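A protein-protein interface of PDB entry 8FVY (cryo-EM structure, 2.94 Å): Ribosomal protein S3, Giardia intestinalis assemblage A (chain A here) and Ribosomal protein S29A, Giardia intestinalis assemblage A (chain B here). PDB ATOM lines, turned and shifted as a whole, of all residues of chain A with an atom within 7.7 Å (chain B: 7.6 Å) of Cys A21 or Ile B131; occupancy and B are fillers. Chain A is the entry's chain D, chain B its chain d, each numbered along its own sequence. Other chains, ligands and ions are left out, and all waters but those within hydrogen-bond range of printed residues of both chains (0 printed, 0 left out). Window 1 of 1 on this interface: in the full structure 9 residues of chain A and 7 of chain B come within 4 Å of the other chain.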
ATOM      1  N   SER A  15       4.563 -17.035 -12.814  1.00  0.00           N
ATOM      2  CA  SER A  15       5.900 -16.581 -12.489  1.00  0.00           C
ATOM      3  C   SER A  15       6.091 -16.381 -11.003  1.00  0.00           C
ATOM      4  O   SER A  15       7.224 -16.207 -10.551  1.00  0.00           O
ATOM      5  CB  SER A  15       6.188 -15.286 -13.219  1.00  0.00           C
ATOM      6  OG  SER A  15       7.580 -15.118 -13.408  1.00  0.00           O
ATOM      7  N   LYS A  16       5.013 -16.385 -10.243  1.00  0.00           N
ATOM      8  CA  LYS A  16       5.089 -16.288  -8.802  1.00  0.00           C
ATOM      9  C   LYS A  16       5.203 -17.647  -8.143  1.00  0.00           C
ATOM     10  O   LYS A  16       5.299 -17.719  -6.917  1.00  0.00           O
ATOM     11  CB  LYS A  16       3.866 -15.550  -8.281  1.00  0.00           C
ATOM     12  CG  LYS A  16       4.052 -14.930  -6.944  1.00  0.00           C
ATOM     13  CD  LYS A  16       2.828 -15.148  -6.081  1.00  0.00           C
ATOM     14  CE  LYS A  16       3.113 -14.851  -4.625  1.00  0.00           C
ATOM     15  NZ  LYS A  16       4.385 -15.450  -4.148  1.00  0.00           N
ATOM     16  N   TYR A  17       5.166 -18.712  -8.929  1.00  0.00           N
ATOM     17  CA  TYR A  17       5.413 -20.070  -8.477  1.00  0.00           C
ATOM     18  C   TYR A  17       6.829 -20.492  -8.799  1.00  0.00           C
ATOM     19  O   TYR A  17       7.496 -21.132  -7.983  1.00  0.00           O
ATOM     20  CB  TYR A  17       4.438 -21.024  -9.154  1.00  0.00           C
ATOM     21  CG  TYR A  17       4.285 -22.354  -8.497  1.00  0.00           C
ATOM     22  CD1 TYR A  17       3.439 -22.524  -7.430  1.00  0.00           C
ATOM     23  CD2 TYR A  17       4.963 -23.448  -8.964  1.00  0.00           C
ATOM     24  CE1 TYR A  17       3.297 -23.738  -6.836  1.00  0.00           C
ATOM     25  CE2 TYR A  17       4.824 -24.658  -8.378  1.00  0.00           C
ATOM     26  CZ  TYR A  17       3.990 -24.802  -7.315  1.00  0.00           C
ATOM     27  OH  TYR A  17       3.848 -26.022  -6.721  1.00  0.00           O
ATOM     28  N   LEU A  18       7.287 -20.119  -9.986  1.00  0.00           N
ATOM     29  CA  LEU A  18       8.625 -20.463 -10.430  1.00  0.00           C
ATOM     30  C   LEU A  18       9.686 -19.864  -9.530  1.00  0.00           C
ATOM     31  O   LEU A  18      10.644 -20.541  -9.146  1.00  0.00           O
ATOM     32  CB  LEU A  18       8.810 -19.958 -11.844  1.00  0.00           C
ATOM     33  CG  LEU A  18       9.983 -20.515 -12.623  1.00  0.00           C
ATOM     34  CD1 LEU A  18       9.795 -21.966 -12.899  1.00  0.00           C
ATOM     35  CD2 LEU A  18      10.150 -19.742 -13.888  1.00  0.00           C
ATOM     36  N   ASN A  19       9.539 -18.589  -9.198  1.00  0.00           N
ATOM     37  CA  ASN A  19      10.526 -17.914  -8.372  1.00  0.00           C
ATOM     38  C   ASN A  19      10.691 -18.615  -7.044  1.00  0.00           C
ATOM     39  O   ASN A  19      11.807 -18.762  -6.535  1.00  0.00           O
ATOM     40  CB  ASN A  19      10.095 -16.480  -8.151  1.00  0.00           C
ATOM     41  CG  ASN A  19       9.925 -15.728  -9.433  1.00  0.00           C
ATOM     42  OD1 ASN A  19      10.016 -16.296 -10.517  1.00  0.00           O
ATOM     43  ND2 ASN A  19       9.678 -14.440  -9.322  1.00  0.00           N
ATOM     44  N   ASP A  20       9.586 -19.040  -6.462  1.00  0.00           N
ATOM     45  CA  ASP A  20       9.603 -19.664  -5.158  1.00  0.00           C
ATOM     46  C   ASP A  20      10.130 -21.086  -5.201  1.00  0.00           C
ATOM     47  O   ASP A  20      10.686 -21.565  -4.209  1.00  0.00           O
ATOM     48  CB  ASP A  20       8.203 -19.596  -4.590  1.00  0.00           C
ATOM     49  CG  ASP A  20       7.775 -18.180  -4.332  1.00  0.00           C
ATOM     50  OD1 ASP A  20       8.043 -17.324  -5.198  1.00  0.00           O
ATOM     51  OD2 ASP A  20       7.188 -17.912  -3.267  1.00  0.00           O
ATOM     52  N   CYS A  21       9.959 -21.771  -6.323  1.00  0.00           N
ATOM     53  CA  CYS A  21      10.596 -23.067  -6.487  1.00  0.00           C
ATOM     54  C   CYS A  21      12.105 -22.926  -6.524  1.00  0.00           C
ATOM     55  O   CYS A  21      12.831 -23.759  -5.974  1.00  0.00           O
ATOM     56  CB  CYS A  21      10.085 -23.733  -7.750  1.00  0.00           C
ATOM     57  SG  CYS A  21       8.429 -24.402  -7.625  1.00  0.00           S
ATOM     58  N   ILE A  22      12.597 -21.881  -7.181  1.00  0.00           N
ATOM     59  CA  ILE A  22      14.024 -21.606  -7.208  1.00  0.00           C
ATOM     60  C   ILE A  22      14.530 -21.221  -5.830  1.00  0.00           C
ATOM     61  O   ILE A  22      15.580 -21.690  -5.383  1.00  0.00           O
ATOM     62  CB  ILE A  22      14.313 -20.505  -8.229  1.00  0.00           C
ATOM     63  CG1 ILE A  22      14.062 -21.025  -9.628  1.00  0.00           C
ATOM     64  CG2 ILE A  22      15.699 -20.046  -8.096  1.00  0.00           C
ATOM     65  CD1 ILE A  22      13.859 -19.974 -10.630  1.00  0.00           C
ATOM     66  N   MET A  23      13.800 -20.353  -5.143  1.00  0.00           N
ATOM     67  CA  MET A  23      14.195 -19.942  -3.808  1.00  0.00           C
ATOM     68  C   MET A  23      14.420 -21.141  -2.906  1.00  0.00           C
ATOM     69  O   MET A  23      15.246 -21.087  -1.993  1.00  0.00           O
ATOM     70  CB  MET A  23      13.116 -19.033  -3.235  1.00  0.00           C
ATOM     71  CG  MET A  23      13.401 -18.448  -1.883  1.00  0.00           C
ATOM     72  SD  MET A  23      11.905 -18.157  -0.931  1.00  0.00           S
ATOM     73  CE  MET A  23      11.046 -17.041  -2.029  1.00  0.00           C
ATOM     74  N   GLU A  24      13.702 -22.227  -3.155  1.00  0.00           N
ATOM     75  CA  GLU A  24      13.830 -23.429  -2.346  1.00  0.00           C
ATOM     76  C   GLU A  24      15.164 -24.121  -2.567  1.00  0.00           C
ATOM     77  O   GLU A  24      15.737 -24.696  -1.637  1.00  0.00           O
ATOM     78  CB  GLU A  24      12.691 -24.367  -2.688  1.00  0.00           C
ATOM     79  CG  GLU A  24      12.238 -25.220  -1.559  1.00  0.00           C
ATOM     80  CD  GLU A  24      11.525 -26.463  -2.029  1.00  0.00           C
ATOM     81  OE1 GLU A  24      11.870 -27.565  -1.557  1.00  0.00           O
ATOM     82  OE2 GLU A  24      10.614 -26.337  -2.872  1.00  0.00           O
ATOM     83  N   ALA A  25      15.653 -24.105  -3.800  1.00  0.00           N
ATOM     84  CA  ALA A  25      16.869 -24.822  -4.130  1.00  0.00           C
ATOM     85  C   ALA A  25      18.092 -24.178  -3.506  1.00  0.00           C
ATOM     86  O   ALA A  25      19.010 -24.869  -3.043  1.00  0.00           O
ATOM     87  CB  ALA A  25      17.010 -24.872  -5.632  1.00  0.00           C
ATOM     88  N   GLU A  26      18.134 -22.853  -3.508  1.00  0.00           N
ATOM     89  CA  GLU A  26      19.221 -22.159  -2.849  1.00  0.00           C
ATOM     90  C   GLU A  26      19.287 -22.541  -1.384  1.00  0.00           C
ATOM     91  O   GLU A  26      20.372 -22.688  -0.814  1.00  0.00           O
ATOM     92  CB  GLU A  26      19.038 -20.664  -3.021  1.00  0.00           C
ATOM     93  CG  GLU A  26      20.227 -19.867  -2.604  1.00  0.00           C
ATOM     94  CD  GLU A  26      20.223 -18.468  -3.154  1.00  0.00           C
ATOM     95  OE1 GLU A  26      19.175 -18.034  -3.669  1.00  0.00           O
ATOM     96  OE2 GLU A  26      21.273 -17.800  -3.073  1.00  0.00           O
ATOM     97  N   LEU A  27      18.133 -22.739  -0.764  1.00  0.00           N
ATOM     98  CA  LEU A  27      18.099 -23.149   0.628  1.00  0.00           C
ATOM     99  C   LEU A  27      18.620 -24.560   0.794  1.00  0.00           C
ATOM    100  O   LEU A  27      19.312 -24.863   1.766  1.00  0.00           O
ATOM    101  CB  LEU A  27      16.682 -23.051   1.144  1.00  0.00           C
ATOM    102  CG  LEU A  27      16.103 -21.648   1.155  1.00  0.00           C
ATOM    103  CD1 LEU A  27      14.659 -21.701   1.454  1.00  0.00           C
ATOM    104  CD2 LEU A  27      16.803 -20.797   2.157  1.00  0.00           C
ATOM    105  N   LEU A  45       8.737 -25.710   1.618  1.00  0.00           N
ATOM    106  CA  LEU A  45       8.347 -24.326   1.787  1.00  0.00           C
ATOM    107  C   LEU A  45       6.840 -24.181   1.645  1.00  0.00           C
ATOM    108  O   LEU A  45       6.165 -25.026   1.056  1.00  0.00           O
ATOM    109  CB  LEU A  45       9.082 -23.450   0.783  1.00  0.00           C
ATOM    110  CG  LEU A  45       8.636 -22.012   0.596  1.00  0.00           C
ATOM    111  CD1 LEU A  45       9.837 -21.158   0.298  1.00  0.00           C
ATOM    112  CD2 LEU A  45       7.652 -21.923  -0.529  1.00  0.00           C
ATOM    113  N   ILE B 104      23.981 -18.971 -10.272  1.00  0.00           N
ATOM    114  CA  ILE B 104      24.597 -20.046  -9.525  1.00  0.00           C
ATOM    115  C   ILE B 104      26.115 -20.021  -9.648  1.00  0.00           C
ATOM    116  O   ILE B 104      26.821 -20.020  -8.646  1.00  0.00           O
ATOM    117  CB  ILE B 104      24.026 -21.386 -10.008  1.00  0.00           C
ATOM    118  CG1 ILE B 104      22.514 -21.323 -10.007  1.00  0.00           C
ATOM    119  CG2 ILE B 104      24.477 -22.491  -9.159  1.00  0.00           C
ATOM    120  CD1 ILE B 104      21.874 -22.518 -10.480  1.00  0.00           C
ATOM    121  N   LEU B 117      14.659 -17.245 -15.757  1.00  0.00           N
ATOM    122  CA  LEU B 117      15.491 -18.192 -15.037  1.00  0.00           C
ATOM    123  C   LEU B 117      16.867 -17.619 -14.728  1.00  0.00           C
ATOM    124  O   LEU B 117      17.178 -17.305 -13.578  1.00  0.00           O
ATOM    125  CB  LEU B 117      15.640 -19.450 -15.871  1.00  0.00           C
ATOM    126  CG  LEU B 117      14.588 -20.530 -15.749  1.00  0.00           C
ATOM    127  CD1 LEU B 117      14.920 -21.598 -16.712  1.00  0.00           C
ATOM    128  CD2 LEU B 117      14.540 -21.098 -14.381  1.00  0.00           C
ATOM    129  N   ILE B 119      19.988 -19.186 -15.631  1.00  0.00           N
ATOM    130  CA  ILE B 119      20.765 -20.345 -15.239  1.00  0.00           C
ATOM    131  C   ILE B 119      21.491 -20.858 -16.468  1.00  0.00           C
ATOM    132  O   ILE B 119      20.893 -20.976 -17.539  1.00  0.00           O
ATOM    133  CB  ILE B 119      19.869 -21.437 -14.645  1.00  0.00           C
ATOM    134  CG1 ILE B 119      19.034 -20.869 -13.524  1.00  0.00           C
ATOM    135  CG2 ILE B 119      20.678 -22.502 -14.068  1.00  0.00           C
ATOM    136  CD1 ILE B 119      18.009 -21.778 -13.066  1.00  0.00           C
ATOM    137  N   CYS B 123      25.018 -25.564 -15.459  1.00  0.00           N
ATOM    138  CA  CYS B 123      24.608 -25.358 -14.081  1.00  0.00           C
ATOM    139  C   CYS B 123      23.126 -25.660 -13.864  1.00  0.00           C
ATOM    140  O   CYS B 123      22.601 -25.337 -12.801  1.00  0.00           O
ATOM    141  CB  CYS B 123      24.993 -23.915 -13.672  1.00  0.00           C
ATOM    142  SG  CYS B 123      26.711 -23.717 -13.098  1.00  0.00           S
ATOM    143  N   PHE B 124      22.471 -26.337 -14.815  1.00  0.00           N
ATOM    144  CA  PHE B 124      21.030 -26.533 -14.847  1.00  0.00           C
ATOM    145  C   PHE B 124      20.602 -27.977 -14.664  1.00  0.00           C
ATOM    146  O   PHE B 124      19.682 -28.260 -13.893  1.00  0.00           O
ATOM    147  CB  PHE B 124      20.496 -26.022 -16.183  1.00  0.00           C
ATOM    148  CG  PHE B 124      19.031 -26.254 -16.392  1.00  0.00           C
ATOM    149  CD1 PHE B 124      18.091 -25.474 -15.774  1.00  0.00           C
ATOM    150  CD2 PHE B 124      18.602 -27.248 -17.226  1.00  0.00           C
ATOM    151  CE1 PHE B 124      16.769 -25.691 -15.970  1.00  0.00           C
ATOM    152  CE2 PHE B 124      17.264 -27.465 -17.419  1.00  0.00           C
ATOM    153  CZ  PHE B 124      16.359 -26.682 -16.788  1.00  0.00           C
ATOM    154  N   GLU B 126      21.919 -30.231 -13.057  1.00  0.00           N
ATOM    155  CA  GLU B 126      22.078 -30.682 -11.686  1.00  0.00           C
ATOM    156  C   GLU B 126      20.866 -30.324 -10.838  1.00  0.00           C
ATOM    157  O   GLU B 126      20.295 -31.188 -10.164  1.00  0.00           O
ATOM    158  CB  GLU B 126      23.338 -30.073 -11.077  1.00  0.00           C
ATOM    159  CG  GLU B 126      24.638 -30.463 -11.748  1.00  0.00           C
ATOM    160  CD  GLU B 126      24.819 -29.820 -13.097  1.00  0.00           C
ATOM    161  OE1 GLU B 126      24.162 -28.791 -13.346  1.00  0.00           O
ATOM    162  OE2 GLU B 126      25.625 -30.332 -13.903  1.00  0.00           O
ATOM    163  N   ASN B 127      20.448 -29.068 -10.880  1.00  0.00           N
ATOM    164  CA  ASN B 127      19.412 -28.555 -10.002  1.00  0.00           C
ATOM    165  C   ASN B 127      18.015 -28.689 -10.584  1.00  0.00           C
ATOM    166  O   ASN B 127      17.037 -28.331  -9.916  1.00  0.00           O
ATOM    167  CB  ASN B 127      19.713 -27.094  -9.682  1.00  0.00           C
ATOM    168  CG  ASN B 127      20.937 -26.929  -8.822  1.00  0.00           C
ATOM    169  OD1 ASN B 127      20.864 -26.963  -7.597  1.00  0.00           O
ATOM    170  ND2 ASN B 127      22.072 -26.741  -9.460  1.00  0.00           N
ATOM    171  N   ALA B 128      17.901 -29.223 -11.794  1.00  0.00           N
ATOM    172  CA  ALA B 128      16.616 -29.301 -12.462  1.00  0.00           C
ATOM    173  C   ALA B 128      15.627 -30.170 -11.708  1.00  0.00           C
ATOM    174  O   ALA B 128      14.437 -29.848 -11.652  1.00  0.00           O
ATOM    175  CB  ALA B 128      16.809 -29.839 -13.860  1.00  0.00           C
ATOM    176  N   GLY B 129      16.084 -31.283 -11.152  1.00  0.00           N
ATOM    177  CA  GLY B 129      15.176 -32.148 -10.428  1.00  0.00           C
ATOM    178  C   GLY B 129      14.665 -31.502  -9.163  1.00  0.00           C
ATOM    179  O   GLY B 129      13.495 -31.649  -8.800  1.00  0.00           O
ATOM    180  N   LYS B 130      15.540 -30.786  -8.466  1.00  0.00           N
ATOM    181  CA  LYS B 130      15.097 -30.045  -7.298  1.00  0.00           C
ATOM    182  C   LYS B 130      14.048 -29.018  -7.676  1.00  0.00           C
ATOM    183  O   LYS B 130      13.030 -28.876  -6.992  1.00  0.00           O
ATOM    184  CB  LYS B 130      16.280 -29.366  -6.630  1.00  0.00           C
ATOM    185  CG  LYS B 130      16.296 -29.536  -5.145  1.00  0.00           C
ATOM    186  CD  LYS B 130      15.074 -28.905  -4.535  1.00  0.00           C
ATOM    187  CE  LYS B 130      15.053 -29.003  -3.034  1.00  0.00           C
ATOM    188  NZ  LYS B 130      13.688 -28.806  -2.533  1.00  0.00           N
ATOM    189  N   ILE B 131      14.277 -28.296  -8.765  1.00  0.00           N
ATOM    190  CA  ILE B 131      13.340 -27.258  -9.168  1.00  0.00           C
ATOM    191  C   ILE B 131      11.993 -27.857  -9.536  1.00  0.00           C
ATOM    192  O   ILE B 131      10.942 -27.321  -9.172  1.00  0.00           O
ATOM    193  CB  ILE B 131      13.946 -26.443 -10.316  1.00  0.00           C
ATOM    194  CG1 ILE B 131      15.157 -25.706  -9.786  1.00  0.00           C
ATOM    195  CG2 ILE B 131      12.971 -25.457 -10.869  1.00  0.00           C
ATOM    196  CD1 ILE B 131      15.744 -24.784 -10.741  1.00  0.00           C
ATOM    197  N   GLY B 132      11.997 -28.960 -10.269  1.00  0.00           N
ATOM    198  CA  GLY B 132      10.760 -29.628 -10.603  1.00  0.00           C
ATOM    199  C   GLY B 132      10.693 -30.085 -12.037  1.00  0.00           C
ATOM    200  O   GLY B 132       9.801 -30.843 -12.419  1.00  0.00           O
ATOM    201  N   PHE B 133      11.631 -29.617 -12.843  1.00  0.00           N
ATOM    202  CA  PHE B 133      11.769 -30.127 -14.190  1.00  0.00           C
ATOM    203  C   PHE B 133      12.102 -31.607 -14.159  1.00  0.00           C
ATOM    204  O   PHE B 133      12.978 -32.048 -13.413  1.00  0.00           O
ATOM    205  CB  PHE B 133      12.863 -29.382 -14.916  1.00  0.00           C
ATOM    206  CG  PHE B 133      12.510 -27.999 -15.301  1.00  0.00           C
ATOM    207  CD1 PHE B 133      12.635 -26.971 -14.415  1.00  0.00           C
ATOM    208  CD2 PHE B 133      12.071 -27.725 -16.564  1.00  0.00           C
ATOM    209  CE1 PHE B 133      12.324 -25.704 -14.783  1.00  0.00           C
ATOM    210  CE2 PHE B 133      11.759 -26.463 -16.929  1.00  0.00           C
ATOM    211  CZ  PHE B 133      11.885 -25.451 -16.041  1.00  0.00           C
ATOM    212  N   VAL B 134      11.409 -32.376 -14.982  1.00  0.00           N
ATOM    213  CA  VAL B 134      11.612 -33.810 -15.048  1.00  0.00           C
ATOM    214  C   VAL B 134      11.649 -34.245 -16.498  1.00  0.00           C
ATOM    215  O   VAL B 134      11.160 -33.550 -17.392  1.00  0.00           O
ATOM    216  CB  VAL B 134      10.519 -34.574 -14.291  1.00  0.00           C
ATOM    217  CG1 VAL B 134      10.620 -34.273 -12.819  1.00  0.00           C
ATOM    218  CG2 VAL B 134       9.162 -34.210 -14.830  1.00  0.00           C
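The backbone carbonyl oxygen (O) of Tyr A17 is in hydrogen-bond range of the side-chain sulfur (SG) of Cys A21.
Of the 14 printed residues of chain B, 3 touch a printed residue of chain A. Hydrophobic or aromatic side chains of chain B within 4 Å of the printed part of chain A: Leu B117. Among the printed residues, 3 pairs touch across the chains. Among the printed residues, Asp or Glu carboxylates within 4 Å of a Lys or Arg side-chain nitrogen of the other chain: Glu A24 with Lys B130.
Cys A21 touches Ile B131 (CB to O, 3.95 Å). Leu B117 touches Ile A22.
The side-chain carboxylate of Glu A24 is in salt-bridge range of the side-chain amino group of Lys B130 (2.4 Å).
Cys A21 touches just one residue of chain B: Ile B131. Ile B131 touches one residue of chain A. Of the printed residues of chain A, Leu B117 touches Ile A22. Of the printed residues of chain B, Glu A24 touches Lys B130 (2.4 Å). Printed residues of chain B within 4 Å of Ile A22: Leu B117 (3.97 Å). Asp A20 touches none of the printed residues of chain B. The nearest residue of chain A that does not touch Ile B131 is Ile A22 (4.3 Å). The nearest printed residue of chain A that does not touch Leu B117 is Leu A18 (4.6 Å).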
